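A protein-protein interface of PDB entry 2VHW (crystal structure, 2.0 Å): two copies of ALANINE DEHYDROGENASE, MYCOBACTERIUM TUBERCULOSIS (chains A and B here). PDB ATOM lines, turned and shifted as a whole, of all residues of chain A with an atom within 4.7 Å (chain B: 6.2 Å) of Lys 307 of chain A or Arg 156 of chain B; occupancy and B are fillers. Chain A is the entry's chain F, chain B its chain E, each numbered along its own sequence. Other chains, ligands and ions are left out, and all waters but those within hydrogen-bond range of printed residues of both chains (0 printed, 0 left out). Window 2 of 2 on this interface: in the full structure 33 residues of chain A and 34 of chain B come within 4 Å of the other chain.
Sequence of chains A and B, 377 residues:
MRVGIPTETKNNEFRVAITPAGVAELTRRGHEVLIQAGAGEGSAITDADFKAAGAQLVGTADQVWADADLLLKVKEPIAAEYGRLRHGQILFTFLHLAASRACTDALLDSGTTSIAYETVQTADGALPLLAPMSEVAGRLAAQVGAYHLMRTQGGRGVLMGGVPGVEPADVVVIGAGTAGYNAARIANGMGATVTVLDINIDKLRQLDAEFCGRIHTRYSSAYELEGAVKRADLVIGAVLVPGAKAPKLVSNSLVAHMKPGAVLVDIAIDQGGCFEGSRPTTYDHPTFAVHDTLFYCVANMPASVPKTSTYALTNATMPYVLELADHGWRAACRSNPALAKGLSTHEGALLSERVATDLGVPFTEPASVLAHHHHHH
No position is printed for both chains.
Of the 9 pairs that touch across the chains among the printed residues, none has its exchanged pair printed and touching as well.
Lys 307 of chain A touches just these residues of chain B: Arg 156 and Gly 157.
Printed residues of chain A within 4 Å of Gly 157 of chain B: Val 305 (3.1 Å), Pro 306 (3.4 Å), Lys 307 (3.1 Å) and Thr 308 (3.9 Å).
Of the printed residues of chain B, Thr 308 of chain A touches Gly 157, Val 158 and Val 166.
Of the printed residues of chain A, Val 166 of chain B touches Thr 308.
Printed residues of chain A within 4 Å of Val 158 of chain B: Val 305 (3.7 Å) and Thr 308 (3.7 Å).
Printed residues of chain B within 4 Å of Val 305 of chain A: Gly 157 (3.1 Å) and Val 158 (3.7 Å).
Leu 149 of chain B touches none of the printed residues of chain A.
Val 263 of chain B touches none of the printed residues of chain A.
The nearest residue of chain B that does not touch Lys 307 of chain A is Val 158 of chain B (4.1 Å).
The nearest printed residue of chain A that does not touch Arg 156 of chain B is Pro 306 of chain A (5.3 Å).
The nearest printed residue of chain B that does not touch Pro 306 of chain A is Arg 156 of chain B (5.3 Å).
Of the 8 printed residues of chain A, 4 touch a printed residue of chain B.
Printed residues of chain A that touch a printed residue of chain B: Val 305, Pro 306, Lys 307 and Thr 308.
Printed residues of chain B that touch a printed residue of chain A: Arg 151, Arg 156, Gly 157, Val 158 and Val 166.
Among the printed residues, no Asp or Glu carboxylate lies within 4 Å of a Lys or Arg side-chain nitrogen of the other chain.
The backbone NH of Gly 157 of chain B sits at hydrogen-bond distance from the backbone carbonyl oxygen of Leu 149 of chain B.
N of Val 158 of chain B lies within hydrogen-bond range of O of Leu 149 of chain B (3.5 Å).
The guanidinium group (NE) of Arg 156 of chain B lies within salt-bridge range of the side-chain carboxylate (OD1) of Asp 233 of chain B, at 3.9 Å.
The backbone carbonyl oxygen (O) of Pro 260 of chain B is in hydrogen-bond range of the guanidinium group (NH1) of Arg 156 of chain B (2.9 Å).
N of Arg 156 of chain B lies within hydrogen-bond range of O of Gly 261 of chain B (2.9 Å).
The side-chain hydroxyl (OG) of Ser 309 of chain A sits at hydrogen-bond distance from the backbone carbonyl oxygen (O) of Val 305 of chain A (3.0 Å).
The backbone carbonyl oxygen of Arg 156 of chain B sits at hydrogen-bond distance from the side-chain amino group of Lys 307 of chain A (2.9 Å).
O of Gly 157 of chain B lies within hydrogen-bond range of N of Lys 307 of chain A (3.1 Å).
O of Val 305 of chain A sits close to O of Gly 157 of chain B, 3.5 Å away.
O of Gly 157 of chain B lies close to N of Pro 306 of chain A (3.4 Å).
Among the printed residues, merely in contact across the chains: Val 305 of chain A with Val 158 of chain B (3.7 Å), Pro 306 of chain A with Arg 151 of chain B (3.8 Å), Thr 308 of chain A with Gly 157 of chain B (3.9 Å), Thr 308 of chain A with Val 158 of chain B (3.7 Å) and Thr 308 of chain A with Val 166 of chain B (3.7 Å).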
ATOM      1  N   SER A  43      19.820  24.012   2.281  1.00  0.00           N
ATOM      2  CA  SER A  43      20.165  25.364   2.723  1.00  0.00           C
ATOM      3  C   SER A  43      19.885  25.582   4.212  1.00  0.00           C
ATOM      4  O   SER A  43      19.871  26.724   4.693  1.00  0.00           O
ATOM      5  CB  SER A  43      19.426  26.396   1.868  1.00  0.00           C
ATOM      6  OG  SER A  43      19.674  26.156   0.493  1.00  0.00           O
ATOM      7  N   ALA A  44      19.675  24.464   4.922  1.00  0.00           N
ATOM      8  CA  ALA A  44      19.402  24.428   6.357  1.00  0.00           C
ATOM      9  C   ALA A  44      18.086  25.118   6.709  1.00  0.00           C
ATOM     10  O   ALA A  44      17.948  25.709   7.783  1.00  0.00           O
ATOM     11  CB  ALA A  44      20.586  24.995   7.170  1.00  0.00           C
ATOM     12  N   VAL A 305      27.746  26.216  -1.927  1.00  0.00           N
ATOM     13  CA  VAL A 305      27.755  27.134  -0.790  1.00  0.00           C
ATOM     14  C   VAL A 305      26.343  27.669  -0.532  1.00  0.00           C
ATOM     15  O   VAL A 305      26.122  28.890  -0.521  1.00  0.00           O
ATOM     16  CB  VAL A 305      28.827  28.267  -0.963  1.00  0.00           C
ATOM     17  CG1 VAL A 305      30.240  27.715  -0.779  1.00  0.00           C
ATOM     18  CG2 VAL A 305      28.711  28.944  -2.335  1.00  0.00           C
ATOM     19  N   PRO A 306      25.371  26.752  -0.303  1.00  0.00           N
ATOM     20  CA  PRO A 306      23.965  27.152  -0.305  1.00  0.00           C
ATOM     21  C   PRO A 306      23.603  28.114   0.839  1.00  0.00           C
ATOM     22  O   PRO A 306      22.675  28.893   0.695  1.00  0.00           O
ATOM     23  CB  PRO A 306      23.221  25.806  -0.144  1.00  0.00           C
ATOM     24  CG  PRO A 306      24.227  24.944   0.604  1.00  0.00           C
ATOM     25  CD  PRO A 306      25.518  25.304  -0.032  1.00  0.00           C
ATOM     26  N   LYS A 307      24.331  28.062   1.953  1.00  0.00           N
ATOM     27  CA  LYS A 307      24.114  29.021   3.036  1.00  0.00           C
ATOM     28  C   LYS A 307      24.356  30.480   2.594  1.00  0.00           C
ATOM     29  O   LYS A 307      23.637  31.387   3.028  1.00  0.00           O
ATOM     30  CB  LYS A 307      24.929  28.644   4.289  1.00  0.00           C
ATOM     31  CG  LYS A 307      24.292  27.493   5.067  1.00  0.00           C
ATOM     32  CD  LYS A 307      24.788  27.455   6.521  1.00  0.00           C
ATOM     33  CE  LYS A 307      24.150  26.286   7.322  1.00  0.00           C
ATOM     34  NZ  LYS A 307      24.457  24.915   6.764  1.00  0.00           N
ATOM     35  N   THR A 308      25.351  30.684   1.723  1.00  0.00           N
ATOM     36  CA  THR A 308      25.615  31.976   1.101  1.00  0.00           C
ATOM     37  C   THR A 308      24.671  32.230  -0.100  1.00  0.00           C
ATOM     38  O   THR A 308      23.984  33.249  -0.163  1.00  0.00           O
ATOM     39  CB  THR A 308      27.091  32.056   0.623  1.00  0.00           C
ATOM     40  OG1 THR A 308      27.954  31.659   1.693  1.00  0.00           O
ATOM     41  CG2 THR A 308      27.477  33.484   0.173  1.00  0.00           C
ATOM     42  N   SER A 309      24.647  31.291  -1.034  1.00  0.00           N
ATOM     43  CA  SER A 309      24.002  31.518  -2.307  1.00  0.00           C
ATOM     44  C   SER A 309      22.477  31.523  -2.307  1.00  0.00           C
ATOM     45  O   SER A 309      21.883  32.256  -3.097  1.00  0.00           O
ATOM     46  CB  SER A 309      24.582  30.578  -3.361  1.00  0.00           C
ATOM     47  OG  SER A 309      24.438  29.255  -2.921  1.00  0.00           O
ATOM     48  N   TYR A 311      20.502  32.733   0.053  1.00  0.00           N
ATOM     49  CA  TYR A 311      20.185  34.074   0.526  1.00  0.00           C
ATOM     50  C   TYR A 311      20.590  35.165  -0.458  1.00  0.00           C
ATOM     51  O   TYR A 311      19.821  36.077  -0.698  1.00  0.00           O
ATOM     52  CB  TYR A 311      20.762  34.295   1.927  1.00  0.00           C
ATOM     53  CG  TYR A 311      20.043  33.416   2.903  1.00  0.00           C
ATOM     54  CD1 TYR A 311      18.848  33.833   3.483  1.00  0.00           C
ATOM     55  CD2 TYR A 311      20.511  32.141   3.195  1.00  0.00           C
ATOM     56  CE1 TYR A 311      18.148  33.023   4.357  1.00  0.00           C
ATOM     57  CE2 TYR A 311      19.809  31.307   4.074  1.00  0.00           C
ATOM     58  CZ  TYR A 311      18.631  31.759   4.654  1.00  0.00           C
ATOM     59  OH  TYR A 311      17.912  30.949   5.524  1.00  0.00           O
ATOM     60  N   HIS B 148      37.012  22.582   1.888  1.00  0.00           N
ATOM     61  CA  HIS B 148      36.235  21.666   2.696  1.00  0.00           C
ATOM     62  C   HIS B 148      34.997  22.289   3.351  1.00  0.00           C
ATOM     63  O   HIS B 148      34.128  21.569   3.838  1.00  0.00           O
ATOM     64  CB  HIS B 148      37.119  20.881   3.670  1.00  0.00           C
ATOM     65  CG  HIS B 148      38.015  19.912   2.974  1.00  0.00           C
ATOM     66  ND1 HIS B 148      37.601  18.645   2.620  1.00  0.00           N
ATOM     67  CD2 HIS B 148      39.277  20.044   2.501  1.00  0.00           C
ATOM     68  CE1 HIS B 148      38.585  18.027   1.988  1.00  0.00           C
ATOM     69  NE2 HIS B 148      39.614  18.853   1.905  1.00  0.00           N
ATOM     70  N   LEU B 149      34.927  23.621   3.349  1.00  0.00           N
ATOM     71  CA  LEU B 149      33.728  24.338   3.785  1.00  0.00           C
ATOM     72  C   LEU B 149      32.550  24.224   2.787  1.00  0.00           C
ATOM     73  O   LEU B 149      31.417  24.554   3.125  1.00  0.00           O
ATOM     74  CB  LEU B 149      34.050  25.816   4.072  1.00  0.00           C
ATOM     75  CG  LEU B 149      34.518  26.210   5.483  1.00  0.00           C
ATOM     76  CD1 LEU B 149      34.826  27.703   5.513  1.00  0.00           C
ATOM     77  CD2 LEU B 149      33.472  25.833   6.569  1.00  0.00           C
ATOM     78  N   MET B 150      32.818  23.759   1.571  1.00  0.00           N
ATOM     79  CA  MET B 150      31.786  23.561   0.562  1.00  0.00           C
ATOM     80  C   MET B 150      30.887  22.392   0.981  1.00  0.00           C
ATOM     81  O   MET B 150      31.377  21.387   1.501  1.00  0.00           O
ATOM     82  CB  MET B 150      32.406  23.280  -0.797  1.00  0.00           C
ATOM     83  CG  MET B 150      33.303  24.424  -1.348  1.00  0.00           C
ATOM     84  SD  MET B 150      33.675  24.189  -3.103  1.00  0.00           S
ATOM     85  CE  MET B 150      34.833  22.887  -3.014  1.00  0.00           C
ATOM     86  N   ARG B 151      29.581  22.530   0.745  1.00  0.00           N
ATOM     87  CA  ARG B 151      28.585  21.521   1.155  1.00  0.00           C
ATOM     88  C   ARG B 151      28.826  20.191   0.424  1.00  0.00           C
ATOM     89  O   ARG B 151      28.548  19.116   0.951  1.00  0.00           O
ATOM     90  CB  ARG B 151      27.158  22.064   0.934  1.00  0.00           C
ATOM     91  CG  ARG B 151      25.983  21.110   1.266  1.00  0.00           C
ATOM     92  CD  ARG B 151      25.924  20.691   2.752  1.00  0.00           C
ATOM     93  NE  ARG B 151      24.773  19.819   3.008  1.00  0.00           N
ATOM     94  CZ  ARG B 151      24.767  18.497   2.826  1.00  0.00           C
ATOM     95  NH1 ARG B 151      25.863  17.863   2.406  1.00  0.00           N
ATOM     96  NH2 ARG B 151      23.656  17.800   3.071  1.00  0.00           N
ATOM     97  N   GLY B 154      30.873  17.885   2.458  1.00  0.00           N
ATOM     98  CA  GLY B 154      30.327  17.600   3.785  1.00  0.00           C
ATOM     99  C   GLY B 154      30.376  18.802   4.713  1.00  0.00           C
ATOM    100  O   GLY B 154      29.897  18.729   5.847  1.00  0.00           O
ATOM    101  N   GLY B 155      30.941  19.910   4.230  1.00  0.00           N
ATOM    102  CA  GLY B 155      31.103  21.123   5.028  1.00  0.00           C
ATOM    103  C   GLY B 155      29.828  21.903   5.262  1.00  0.00           C
ATOM    104  O   GLY B 155      28.791  21.583   4.712  1.00  0.00           O
ATOM    105  N   ARG B 156      29.927  22.963   6.057  1.00  0.00           N
ATOM    106  CA  ARG B 156      28.785  23.840   6.371  1.00  0.00           C
ATOM    107  C   ARG B 156      28.099  24.466   5.143  1.00  0.00           C
ATOM    108  O   ARG B 156      26.895  24.726   5.163  1.00  0.00           O
ATOM    109  CB  ARG B 156      29.234  24.920   7.376  1.00  0.00           C
ATOM    110  CG  ARG B 156      28.088  25.706   7.977  1.00  0.00           C
ATOM    111  CD  ARG B 156      28.411  26.281   9.352  1.00  0.00           C
ATOM    112  NE  ARG B 156      27.256  27.009   9.883  1.00  0.00           N
ATOM    113  CZ  ARG B 156      26.217  26.439  10.507  1.00  0.00           C
ATOM    114  NH1 ARG B 156      26.156  25.111  10.689  1.00  0.00           N
ATOM    115  NH2 ARG B 156      25.217  27.197  10.956  1.00  0.00           N
ATOM    116  N   GLY B 157      28.845  24.698   4.064  1.00  0.00           N
ATOM    117  CA  GLY B 157      28.252  25.270   2.856  1.00  0.00           C
ATOM    118  C   GLY B 157      28.266  26.791   2.863  1.00  0.00           C
ATOM    119  O   GLY B 157      27.301  27.433   2.418  1.00  0.00           O
ATOM    120  N   VAL B 158      29.377  27.353   3.348  1.00  0.00           N
ATOM    121  CA  VAL B 158      29.578  28.790   3.451  1.00  0.00           C
ATOM    122  C   VAL B 158      30.757  29.173   2.539  1.00  0.00           C
ATOM    123  O   VAL B 158      31.798  28.485   2.542  1.00  0.00           O
ATOM    124  CB  VAL B 158      29.890  29.224   4.923  1.00  0.00           C
ATOM    125  CG1 VAL B 158      30.106  30.718   5.007  1.00  0.00           C
ATOM    126  CG2 VAL B 158      28.724  28.823   5.870  1.00  0.00           C
ATOM    127  N   VAL B 166      25.608  39.364   2.368  1.00  0.00           N
ATOM    128  CA  VAL B 166      25.613  38.008   2.953  1.00  0.00           C
ATOM    129  C   VAL B 166      26.932  37.773   3.716  1.00  0.00           C
ATOM    130  O   VAL B 166      28.009  38.040   3.178  1.00  0.00           O
ATOM    131  CB  VAL B 166      25.418  36.935   1.842  1.00  0.00           C
ATOM    132  CG1 VAL B 166      25.383  35.565   2.425  1.00  0.00           C
ATOM    133  CG2 VAL B 166      24.116  37.203   1.060  1.00  0.00           C
ATOM    134  N   ALA B 232      33.253  29.723  15.159  1.00  0.00           N
ATOM    135  CA  ALA B 232      34.032  29.531  13.925  1.00  0.00           C
ATOM    136  C   ALA B 232      33.394  28.598  12.892  1.00  0.00           C
ATOM    137  O   ALA B 232      32.805  27.587  13.240  1.00  0.00           O
ATOM    138  CB  ALA B 232      35.421  29.027  14.269  1.00  0.00           C
ATOM    139  N   ASP B 233      33.536  28.953  11.615  1.00  0.00           N
ATOM    140  CA  ASP B 233      33.248  28.047  10.496  1.00  0.00           C
ATOM    141  C   ASP B 233      34.472  27.193  10.178  1.00  0.00           C
ATOM    142  O   ASP B 233      34.359  26.058   9.704  1.00  0.00           O
ATOM    143  CB  ASP B 233      32.884  28.853   9.256  1.00  0.00           C
ATOM    144  CG  ASP B 233      31.611  29.644   9.440  1.00  0.00           C
ATOM    145  OD1 ASP B 233      30.588  29.029   9.793  1.00  0.00           O
ATOM    146  OD2 ASP B 233      31.623  30.872   9.253  1.00  0.00           O
ATOM    147  N   LYS B 259      29.513  24.556  15.361  1.00  0.00           N
ATOM    148  CA  LYS B 259      28.508  24.541  14.300  1.00  0.00           C
ATOM    149  C   LYS B 259      28.661  23.275  13.457  1.00  0.00           C
ATOM    150  O   LYS B 259      29.784  22.887  13.139  1.00  0.00           O
ATOM    151  CB  LYS B 259      28.699  25.755  13.397  1.00  0.00           C
ATOM    152  CG  LYS B 259      28.542  27.113  14.063  1.00  0.00           C
ATOM    153  CD  LYS B 259      29.144  28.177  13.157  1.00  0.00           C
ATOM    154  CE  LYS B 259      28.877  29.569  13.662  1.00  0.00           C
ATOM    155  NZ  LYS B 259      29.430  30.564  12.689  1.00  0.00           N
ATOM    156  N   PRO B 260      27.539  22.610  13.102  1.00  0.00           N
ATOM    157  CA  PRO B 260      27.659  21.449  12.208  1.00  0.00           C
ATOM    158  C   PRO B 260      28.306  21.843  10.878  1.00  0.00           C
ATOM    159  O   PRO B 260      27.950  22.860  10.305  1.00  0.00           O
ATOM    160  CB  PRO B 260      26.205  21.030  11.988  1.00  0.00           C
ATOM    161  CG  PRO B 260      25.503  21.506  13.226  1.00  0.00           C
ATOM    162  CD  PRO B 260      26.139  22.849  13.487  1.00  0.00           C
ATOM    163  N   GLY B 261      29.248  21.036  10.403  1.00  0.00           N
ATOM    164  CA  GLY B 261      29.889  21.296   9.121  1.00  0.00           C
ATOM    165  C   GLY B 261      31.116  22.194   9.217  1.00  0.00           C
ATOM    166  O   GLY B 261      31.750  22.482   8.195  1.00  0.00           O
ATOM    167  N   ALA B 262      31.442  22.655  10.428  1.00  0.00           N
ATOM    168  CA  ALA B 262      32.711  23.384  10.671  1.00  0.00           C
ATOM    169  C   ALA B 262      33.905  22.504  10.330  1.00  0.00           C
ATOM    170  O   ALA B 262      33.841  21.277  10.484  1.00  0.00           O
ATOM    171  CB  ALA B 262      32.799  23.883  12.124  1.00  0.00           C
ATOM    172  N   VAL B 263      34.984  23.137   9.877  1.00  0.00           N
ATOM    173  CA  VAL B 263      36.211  22.469   9.447  1.00  0.00           C
ATOM    174  C   VAL B 263      37.332  22.874  10.402  1.00  0.00           C
ATOM    175  O   VAL B 263      37.430  24.034  10.785  1.00  0.00           O
ATOM    176  CB  VAL B 263      36.565  22.851   7.976  1.00  0.00           C
ATOM    177  CG1 VAL B 263      37.879  22.234   7.511  1.00  0.00           C
ATOM    178  CG2 VAL B 263      35.429  22.445   7.022  1.00  0.00           C
